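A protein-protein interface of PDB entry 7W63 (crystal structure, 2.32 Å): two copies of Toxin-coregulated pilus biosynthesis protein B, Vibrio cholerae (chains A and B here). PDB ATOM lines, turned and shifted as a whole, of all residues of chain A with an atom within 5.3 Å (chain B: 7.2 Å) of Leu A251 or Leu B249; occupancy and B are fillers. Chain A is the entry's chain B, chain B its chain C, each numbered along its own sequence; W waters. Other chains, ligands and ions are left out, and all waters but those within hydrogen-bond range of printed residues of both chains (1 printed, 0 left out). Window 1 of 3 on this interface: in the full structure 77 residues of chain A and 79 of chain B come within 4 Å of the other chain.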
ATOM      1  N   LEU A 236     -15.576  14.661  18.924  1.00  0.00           N
ATOM      2  CA  LEU A 236     -16.867  14.992  19.488  1.00  0.00           C
ATOM      3  C   LEU A 236     -17.921  14.999  18.382  1.00  0.00           C
ATOM      4  O   LEU A 236     -17.580  15.010  17.203  1.00  0.00           O
ATOM      5  CB  LEU A 236     -16.807  16.340  20.210  1.00  0.00           C
ATOM      6  CG  LEU A 236     -16.250  17.563  19.491  1.00  0.00           C
ATOM      7  CD1 LEU A 236     -17.340  18.240  18.666  1.00  0.00           C
ATOM      8  CD2 LEU A 236     -15.671  18.555  20.494  1.00  0.00           C
ATOM      9  N   LEU A 249     -24.865  16.603  22.457  1.00  0.00           N
ATOM     10  CA  LEU A 249     -23.505  17.022  22.107  1.00  0.00           C
ATOM     11  C   LEU A 249     -22.557  16.141  22.904  1.00  0.00           C
ATOM     12  O   LEU A 249     -22.371  16.344  24.114  1.00  0.00           O
ATOM     13  CB  LEU A 249     -23.256  18.503  22.417  1.00  0.00           C
ATOM     14  CG  LEU A 249     -21.826  18.992  22.195  1.00  0.00           C
ATOM     15  CD1 LEU A 249     -21.445  18.885  20.721  1.00  0.00           C
ATOM     16  CD2 LEU A 249     -21.639  20.422  22.705  1.00  0.00           C
ATOM     17  N   ASP A 250     -21.998  15.136  22.239  1.00  0.00           N
ATOM     18  CA  ASP A 250     -21.289  14.071  22.936  1.00  0.00           C
ATOM     19  C   ASP A 250     -19.825  14.442  23.123  1.00  0.00           C
ATOM     20  O   ASP A 250     -19.048  14.417  22.171  1.00  0.00           O
ATOM     21  CB  ASP A 250     -21.424  12.755  22.161  1.00  0.00           C
ATOM     22  CG  ASP A 250     -20.709  11.577  22.840  1.00  0.00           C
ATOM     23  OD1 ASP A 250     -20.126  11.731  23.942  1.00  0.00           O
ATOM     24  OD2 ASP A 250     -20.725  10.482  22.247  1.00  0.00           O
ATOM     25  N   LEU A 251     -19.457  14.763  24.358  1.00  0.00           N
ATOM     26  CA  LEU A 251     -18.092  15.152  24.667  1.00  0.00           C
ATOM     27  C   LEU A 251     -17.364  14.084  25.477  1.00  0.00           C
ATOM     28  O   LEU A 251     -16.302  14.341  26.032  1.00  0.00           O
ATOM     29  CB  LEU A 251     -18.082  16.485  25.420  1.00  0.00           C
ATOM     30  CG  LEU A 251     -18.883  17.618  24.757  1.00  0.00           C
ATOM     31  CD1 LEU A 251     -18.999  18.838  25.663  1.00  0.00           C
ATOM     32  CD2 LEU A 251     -18.275  18.017  23.416  1.00  0.00           C
ATOM     33  N   LYS A 252     -17.914  12.875  25.523  1.00  0.00           N
ATOM     34  CA  LYS A 252     -17.397  11.865  26.445  1.00  0.00           C
ATOM     35  C   LYS A 252     -16.065  11.204  26.070  1.00  0.00           C
ATOM     36  O   LYS A 252     -15.468  10.539  26.905  1.00  0.00           O
ATOM     37  CB  LYS A 252     -18.453  10.791  26.665  1.00  0.00           C
ATOM     38  CG  LYS A 252     -19.615  11.329  27.497  1.00  0.00           C
ATOM     39  CD  LYS A 252     -20.544  10.246  27.982  1.00  0.00           C
ATOM     40  CE  LYS A 252     -21.280   9.621  26.818  1.00  0.00           C
ATOM     41  NZ  LYS A 252     -22.197  10.592  26.188  1.00  0.00           N
ATOM     42  N   GLN A 253     -15.570  11.385  24.848  1.00  0.00           N
ATOM     43  CA  GLN A 253     -14.208  10.925  24.560  1.00  0.00           C
ATOM     44  C   GLN A 253     -13.176  11.835  25.243  1.00  0.00           C
ATOM     45  O   GLN A 253     -12.002  11.491  25.336  1.00  0.00           O
ATOM     46  CB  GLN A 253     -13.954  10.875  23.054  1.00  0.00           C
ATOM     47  CG  GLN A 253     -14.837   9.900  22.336  1.00  0.00           C
ATOM     48  CD  GLN A 253     -14.550   9.811  20.853  1.00  0.00           C
ATOM     49  OE1 GLN A 253     -13.426  10.075  20.398  1.00  0.00           O
ATOM     50  NE2 GLN A 253     -15.573   9.444  20.080  1.00  0.00           N
ATOM     51  N   ILE A 254     -13.611  13.005  25.700  1.00  0.00           N
ATOM     52  CA  ILE A 254     -12.712  13.942  26.364  1.00  0.00           C
ATOM     53  C   ILE A 254     -12.782  13.716  27.876  1.00  0.00           C
ATOM     54  O   ILE A 254     -13.865  13.550  28.424  1.00  0.00           O
ATOM     55  CB  ILE A 254     -13.069  15.411  26.016  1.00  0.00           C
ATOM     56  CG1 ILE A 254     -13.409  15.560  24.539  1.00  0.00           C
ATOM     57  CG2 ILE A 254     -11.931  16.337  26.389  1.00  0.00           C
ATOM     58  CD1 ILE A 254     -12.283  15.212  23.661  1.00  0.00           C
ATOM     59  N   VAL A 256     -11.850  15.867  30.482  1.00  0.00           N
ATOM     60  CA  VAL A 256     -12.417  17.006  31.192  1.00  0.00           C
ATOM     61  C   VAL A 256     -12.845  18.101  30.209  1.00  0.00           C
ATOM     62  O   VAL A 256     -12.071  18.495  29.329  1.00  0.00           O
ATOM     63  CB  VAL A 256     -11.420  17.567  32.234  1.00  0.00           C
ATOM     64  CG1 VAL A 256     -12.055  18.718  33.022  1.00  0.00           C
ATOM     65  CG2 VAL A 256     -10.959  16.471  33.182  1.00  0.00           C
ATOM     66  N   VAL A 257     -14.088  18.556  30.338  1.00  0.00           N
ATOM     67  CA  VAL A 257     -14.535  19.742  29.631  1.00  0.00           C
ATOM     68  C   VAL A 257     -14.291  20.916  30.570  1.00  0.00           C
ATOM     69  O   VAL A 257     -14.849  20.960  31.664  1.00  0.00           O
ATOM     70  CB  VAL A 257     -16.011  19.656  29.203  1.00  0.00           C
ATOM     71  CG1 VAL A 257     -16.481  20.994  28.647  1.00  0.00           C
ATOM     72  CG2 VAL A 257     -16.196  18.566  28.168  1.00  0.00           C
ATOM     73  N   SER A 258     -13.450  21.853  30.140  1.00  0.00           N
ATOM     74  CA  SER A 258     -12.984  22.943  30.999  1.00  0.00           C
ATOM     75  C   SER A 258     -13.551  24.293  30.559  1.00  0.00           C
ATOM     76  O   SER A 258     -13.079  24.903  29.594  1.00  0.00           O
ATOM     77  CB  SER A 258     -11.459  22.987  31.003  1.00  0.00           C
ATOM     78  OG  SER A 258     -10.979  24.031  31.817  1.00  0.00           O
ATOM     79  N   ALA A 259     -14.562  24.748  31.291  1.00  0.00           N
ATOM     80  CA  ALA A 259     -15.267  25.977  30.978  1.00  0.00           C
ATOM     81  C   ALA A 259     -14.838  27.131  31.878  1.00  0.00           C
ATOM     82  O   ALA A 259     -14.221  26.931  32.930  1.00  0.00           O
ATOM     83  CB  ALA A 259     -16.750  25.756  31.099  1.00  0.00           C
ATOM     84  N   PRO B 105     -17.535   5.602  23.597  1.00  0.00           N
ATOM     85  CA  PRO B 105     -18.513   5.987  24.636  1.00  0.00           C
ATOM     86  C   PRO B 105     -19.981   5.889  24.195  1.00  0.00           C
ATOM     87  O   PRO B 105     -20.864   5.706  25.037  1.00  0.00           O
ATOM     88  CB  PRO B 105     -18.155   7.450  24.932  1.00  0.00           C
ATOM     89  CG  PRO B 105     -16.730   7.608  24.486  1.00  0.00           C
ATOM     90  CD  PRO B 105     -16.569   6.681  23.307  1.00  0.00           C
ATOM     91  N   SER B 106     -20.232   6.012  22.896  1.00  0.00           N
ATOM     92  CA  SER B 106     -21.592   6.029  22.379  1.00  0.00           C
ATOM     93  C   SER B 106     -21.807   4.961  21.319  1.00  0.00           C
ATOM     94  O   SER B 106     -22.840   4.947  20.656  1.00  0.00           O
ATOM     95  CB  SER B 106     -21.921   7.394  21.780  1.00  0.00           C
ATOM     96  OG  SER B 106     -21.859   8.395  22.778  1.00  0.00           O
ATOM     97  N   LEU B 236     -11.747  27.346  20.723  1.00  0.00           N
ATOM     98  CA  LEU B 236     -11.732  26.195  21.607  1.00  0.00           C
ATOM     99  C   LEU B 236     -10.755  25.165  21.037  1.00  0.00           C
ATOM    100  O   LEU B 236     -10.464  25.177  19.833  1.00  0.00           O
ATOM    101  CB  LEU B 236     -13.132  25.598  21.772  1.00  0.00           C
ATOM    102  CG  LEU B 236     -13.948  25.257  20.529  1.00  0.00           C
ATOM    103  CD1 LEU B 236     -13.773  23.785  20.183  1.00  0.00           C
ATOM    104  CD2 LEU B 236     -15.431  25.596  20.730  1.00  0.00           C
ATOM    105  N   SER B 237     -10.242  24.284  21.897  1.00  0.00           N
ATOM    106  CA  SER B 237      -9.280  23.276  21.466  1.00  0.00           C
ATOM    107  C   SER B 237      -9.363  21.996  22.313  1.00  0.00           C
ATOM    108  O   SER B 237      -9.860  22.011  23.441  1.00  0.00           O
ATOM    109  CB  SER B 237      -7.861  23.863  21.503  1.00  0.00           C
ATOM    110  OG  SER B 237      -7.409  24.085  22.835  1.00  0.00           O
ATOM    111  N   VAL B 238      -8.911  20.887  21.738  1.00  0.00           N
ATOM    112  CA  VAL B 238      -8.745  19.631  22.465  1.00  0.00           C
ATOM    113  C   VAL B 238      -7.255  19.316  22.558  1.00  0.00           C
ATOM    114  O   VAL B 238      -6.555  19.231  21.539  1.00  0.00           O
ATOM    115  CB  VAL B 238      -9.489  18.472  21.798  1.00  0.00           C
ATOM    116  CG1 VAL B 238      -9.134  17.154  22.490  1.00  0.00           C
ATOM    117  CG2 VAL B 238     -10.998  18.708  21.824  1.00  0.00           C
ATOM    118  N   ARG B 239      -6.771  19.139  23.776  1.00  0.00           N
ATOM    119  CA  ARG B 239      -5.354  18.930  23.993  1.00  0.00           C
ATOM    120  C   ARG B 239      -5.120  17.752  24.932  1.00  0.00           C
ATOM    121  O   ARG B 239      -5.997  17.397  25.724  1.00  0.00           O
ATOM    122  CB  ARG B 239      -4.719  20.206  24.540  1.00  0.00           C
ATOM    123  CG  ARG B 239      -4.320  21.166  23.420  1.00  0.00           C
ATOM    124  CD  ARG B 239      -4.226  22.623  23.869  1.00  0.00           C
ATOM    125  NE  ARG B 239      -4.238  23.538  22.722  1.00  0.00           N
ATOM    126  CZ  ARG B 239      -3.252  24.388  22.419  1.00  0.00           C
ATOM    127  NH1 ARG B 239      -2.159  24.454  23.183  1.00  0.00           N
ATOM    128  NH2 ARG B 239      -3.358  25.180  21.351  1.00  0.00           N
ATOM    129  N   THR B 247      -7.095  14.176  28.479  1.00  0.00           N
ATOM    130  CA  THR B 247      -7.439  15.156  27.458  1.00  0.00           C
ATOM    131  C   THR B 247      -8.302  16.254  28.084  1.00  0.00           C
ATOM    132  O   THR B 247      -8.994  16.017  29.079  1.00  0.00           O
ATOM    133  CB  THR B 247      -8.181  14.521  26.283  1.00  0.00           C
ATOM    134  OG1 THR B 247      -9.243  13.706  26.786  1.00  0.00           O
ATOM    135  CG2 THR B 247      -7.228  13.670  25.443  1.00  0.00           C
ATOM    136  N   GLU B 248      -8.246  17.450  27.509  1.00  0.00           N
ATOM    137  CA  GLU B 248      -9.083  18.556  27.947  1.00  0.00           C
ATOM    138  C   GLU B 248      -9.727  19.239  26.749  1.00  0.00           C
ATOM    139  O   GLU B 248      -9.075  19.461  25.738  1.00  0.00           O
ATOM    140  CB  GLU B 248      -8.271  19.581  28.748  1.00  0.00           C
ATOM    141  CG  GLU B 248      -9.087  20.800  29.193  1.00  0.00           C
ATOM    142  CD  GLU B 248      -8.254  21.870  29.915  1.00  0.00           C
ATOM    143  OE1 GLU B 248      -7.585  22.679  29.236  1.00  0.00           O
ATOM    144  OE2 GLU B 248      -8.274  21.902  31.166  1.00  0.00           O
ATOM    145  N   LEU B 249     -11.011  19.551  26.857  1.00  0.00           N
ATOM    146  CA  LEU B 249     -11.658  20.421  25.890  1.00  0.00           C
ATOM    147  C   LEU B 249     -11.629  21.805  26.511  1.00  0.00           C
ATOM    148  O   LEU B 249     -12.391  22.107  27.421  1.00  0.00           O
ATOM    149  CB  LEU B 249     -13.092  19.960  25.566  1.00  0.00           C
ATOM    150  CG  LEU B 249     -13.964  20.891  24.717  1.00  0.00           C
ATOM    151  CD1 LEU B 249     -13.361  21.105  23.354  1.00  0.00           C
ATOM    152  CD2 LEU B 249     -15.384  20.355  24.558  1.00  0.00           C
ATOM    153  N   ASP B 250     -10.700  22.624  26.050  1.00  0.00           N
ATOM    154  CA  ASP B 250     -10.493  23.939  26.613  1.00  0.00           C
ATOM    155  C   ASP B 250     -11.463  24.941  25.968  1.00  0.00           C
ATOM    156  O   ASP B 250     -11.314  25.306  24.793  1.00  0.00           O
ATOM    157  CB  ASP B 250      -9.028  24.356  26.420  1.00  0.00           C
ATOM    158  CG  ASP B 250      -8.747  25.790  26.872  1.00  0.00           C
ATOM    159  OD1 ASP B 250      -9.702  26.529  27.231  1.00  0.00           O
ATOM    160  OD2 ASP B 250      -7.554  26.182  26.859  1.00  0.00           O
ATOM    161  N   LEU B 251     -12.445  25.368  26.766  1.00  0.00           N
ATOM    162  CA  LEU B 251     -13.455  26.357  26.380  1.00  0.00           C
ATOM    163  C   LEU B 251     -13.310  27.683  27.119  1.00  0.00           C
ATOM    164  O   LEU B 251     -14.190  28.540  27.026  1.00  0.00           O
ATOM    165  CB  LEU B 251     -14.862  25.833  26.644  1.00  0.00           C
ATOM    166  CG  LEU B 251     -15.304  24.479  26.085  1.00  0.00           C
ATOM    167  CD1 LEU B 251     -16.717  24.158  26.582  1.00  0.00           C
ATOM    168  CD2 LEU B 251     -15.233  24.442  24.560  1.00  0.00           C
ATOM    169  N   LYS B 252     -12.215  27.853  27.853  1.00  0.00           N
ATOM    170  CA  LYS B 252     -12.044  29.022  28.729  1.00  0.00           C
ATOM    171  C   LYS B 252     -11.839  30.359  27.990  1.00  0.00           C
ATOM    172  O   LYS B 252     -12.094  31.422  28.555  1.00  0.00           O
ATOM    173  CB  LYS B 252     -10.880  28.782  29.695  1.00  0.00           C
ATOM    174  CG  LYS B 252     -11.139  27.617  30.646  1.00  0.00           C
ATOM    175  CD  LYS B 252     -10.156  27.587  31.817  1.00  0.00           C
ATOM    176  CE  LYS B 252      -8.724  27.298  31.346  1.00  0.00           C
ATOM    177  NZ  LYS B 252      -8.552  25.933  30.785  1.00  0.00           N
ATOM    178  N   LEU B 262     -27.713  19.484  30.548  1.00  0.00           N
ATOM    179  CA  LEU B 262     -26.291  19.245  30.805  1.00  0.00           C
ATOM    180  C   LEU B 262     -26.078  18.027  31.700  1.00  0.00           C
ATOM    181  O   LEU B 262     -26.743  17.891  32.741  1.00  0.00           O
ATOM    182  CB  LEU B 262     -25.658  20.491  31.435  1.00  0.00           C
ATOM    183  CG  LEU B 262     -24.198  20.353  31.882  1.00  0.00           C
ATOM    184  CD1 LEU B 262     -23.269  20.164  30.679  1.00  0.00           C
ATOM    185  CD2 LEU B 262     -23.748  21.524  32.772  1.00  0.00           C
ATOM    186  N   SER B 263     -25.174  17.131  31.301  1.00  0.00           N
ATOM    187  CA  SER B 263     -24.801  15.999  32.159  1.00  0.00           C
ATOM    188  C   SER B 263     -23.310  15.755  32.138  1.00  0.00           C
ATOM    189  O   SER B 263     -22.615  16.135  31.190  1.00  0.00           O
ATOM    190  CB  SER B 263     -25.533  14.714  31.763  1.00  0.00           C
ATOM    191  OG  SER B 263     -24.980  14.119  30.595  1.00  0.00           O
HETATM  192  O   HOH W   1      -9.074  11.310  26.219  1.00  0.00           O
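The backbone carbonyl oxygen (O) of Ser A258 is in hydrogen-bond range of the backbone NH (N) of Leu B251.
The backbone NH of Val A256 is in hydrogen-bond range of the backbone carbonyl oxygen of Thr B247 (3.2 Å).
The side-chain hydroxyl (OG) of Ser A258 sits at hydrogen-bond distance from the side-chain amino group (NZ) of Lys B252 (3.3 Å).
OD2 of Asp A250 lies within hydrogen-bond range of OG of Ser B106 (2.4 Å).
O of Val A256 sits at hydrogen-bond distance from N of Leu B249.
The backbone carbonyl oxygen (O) of Leu B249 sits at hydrogen-bond distance from the backbone NH (N) of Ser A258 (2.9 Å).
The side-chain carboxylate of Glu B248 lies within salt-bridge range of the side-chain amino group of Lys B252, 3.7 Å away.
The side-chain amino group (NZ) of Lys A252 lies within salt-bridge range of the side-chain carboxylate (OD1) of Asp A250.
O of Arg B239 lies within hydrogen-bond range of N of Glu B248.
The backbone carbonyl oxygen (O) of Ser B237 is in hydrogen-bond range of the backbone NH (N) of Asp B250, 2.8 Å away.
The side-chain carboxylate of Asp B250 is in salt-bridge range of the side-chain amino group of Lys B252 (3.8 Å).
Lys A252 touches Pro B105 (CB to CB, 3.8 Å).
Pro B105 touches Gln A253.
CA of Ile A254 touches OG1 of Thr B247, 3.5 Å away.
Ile A254 touches Glu B248.
Ile A254 touches Leu B249.
Val A256 touches Glu B248 (O to CA, 3.3 Å).
C of Val A257 touches O of Leu B249 (3.9 Å).
CG1 of Val A257 touches CD1 of Leu B251, at 3.8 Å.
Ser A258 touches Glu B248.
Ala A259 touches Lys B252.
Leu A251 touches just one residue of chain B: Leu B249.
Printed residues of chain A within 4 Å of Ser B106: Asp A250.
Leu B236 touches none of the printed residues of chain A.
Ser B237 touches none of the printed residues of chain A.
Printed residues of chain A within 4 Å of Val B238: Ile A254 (3.9 Å).
Of the printed residues of chain A, Leu B249 touches Leu A251, Ile A254, Val A256, Val A257 and Ser A258.
The nearest residue of chain A that does not touch Leu B249 is Leu A236 (4.5 Å).
Along chain A the printed residues that touch a printed residue of chain B span positions 250 to 259.
Of the 14 printed residues of chain B, 9 touch a printed residue of chain A.
Along chain B the printed residues that touch a printed residue of chain A span positions 105 to 252.
Among the printed residues, 20 pairs touch across the chains.
Leu A251 touches Leu B249, but with the chains exchanged Leu A249 does not touch Leu B251 (7.3 Å).
Positions printed for both chains: 236, 249, 250, 251 and 252.
Of the 20 pairs that touch across the chains among the printed residues, none has its exchanged pair printed and touching as well.
Water W1 bridges the side-chain hydroxyl (OG1) of Thr B247 and the backbone carbonyl oxygen (O) of Gln A253.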
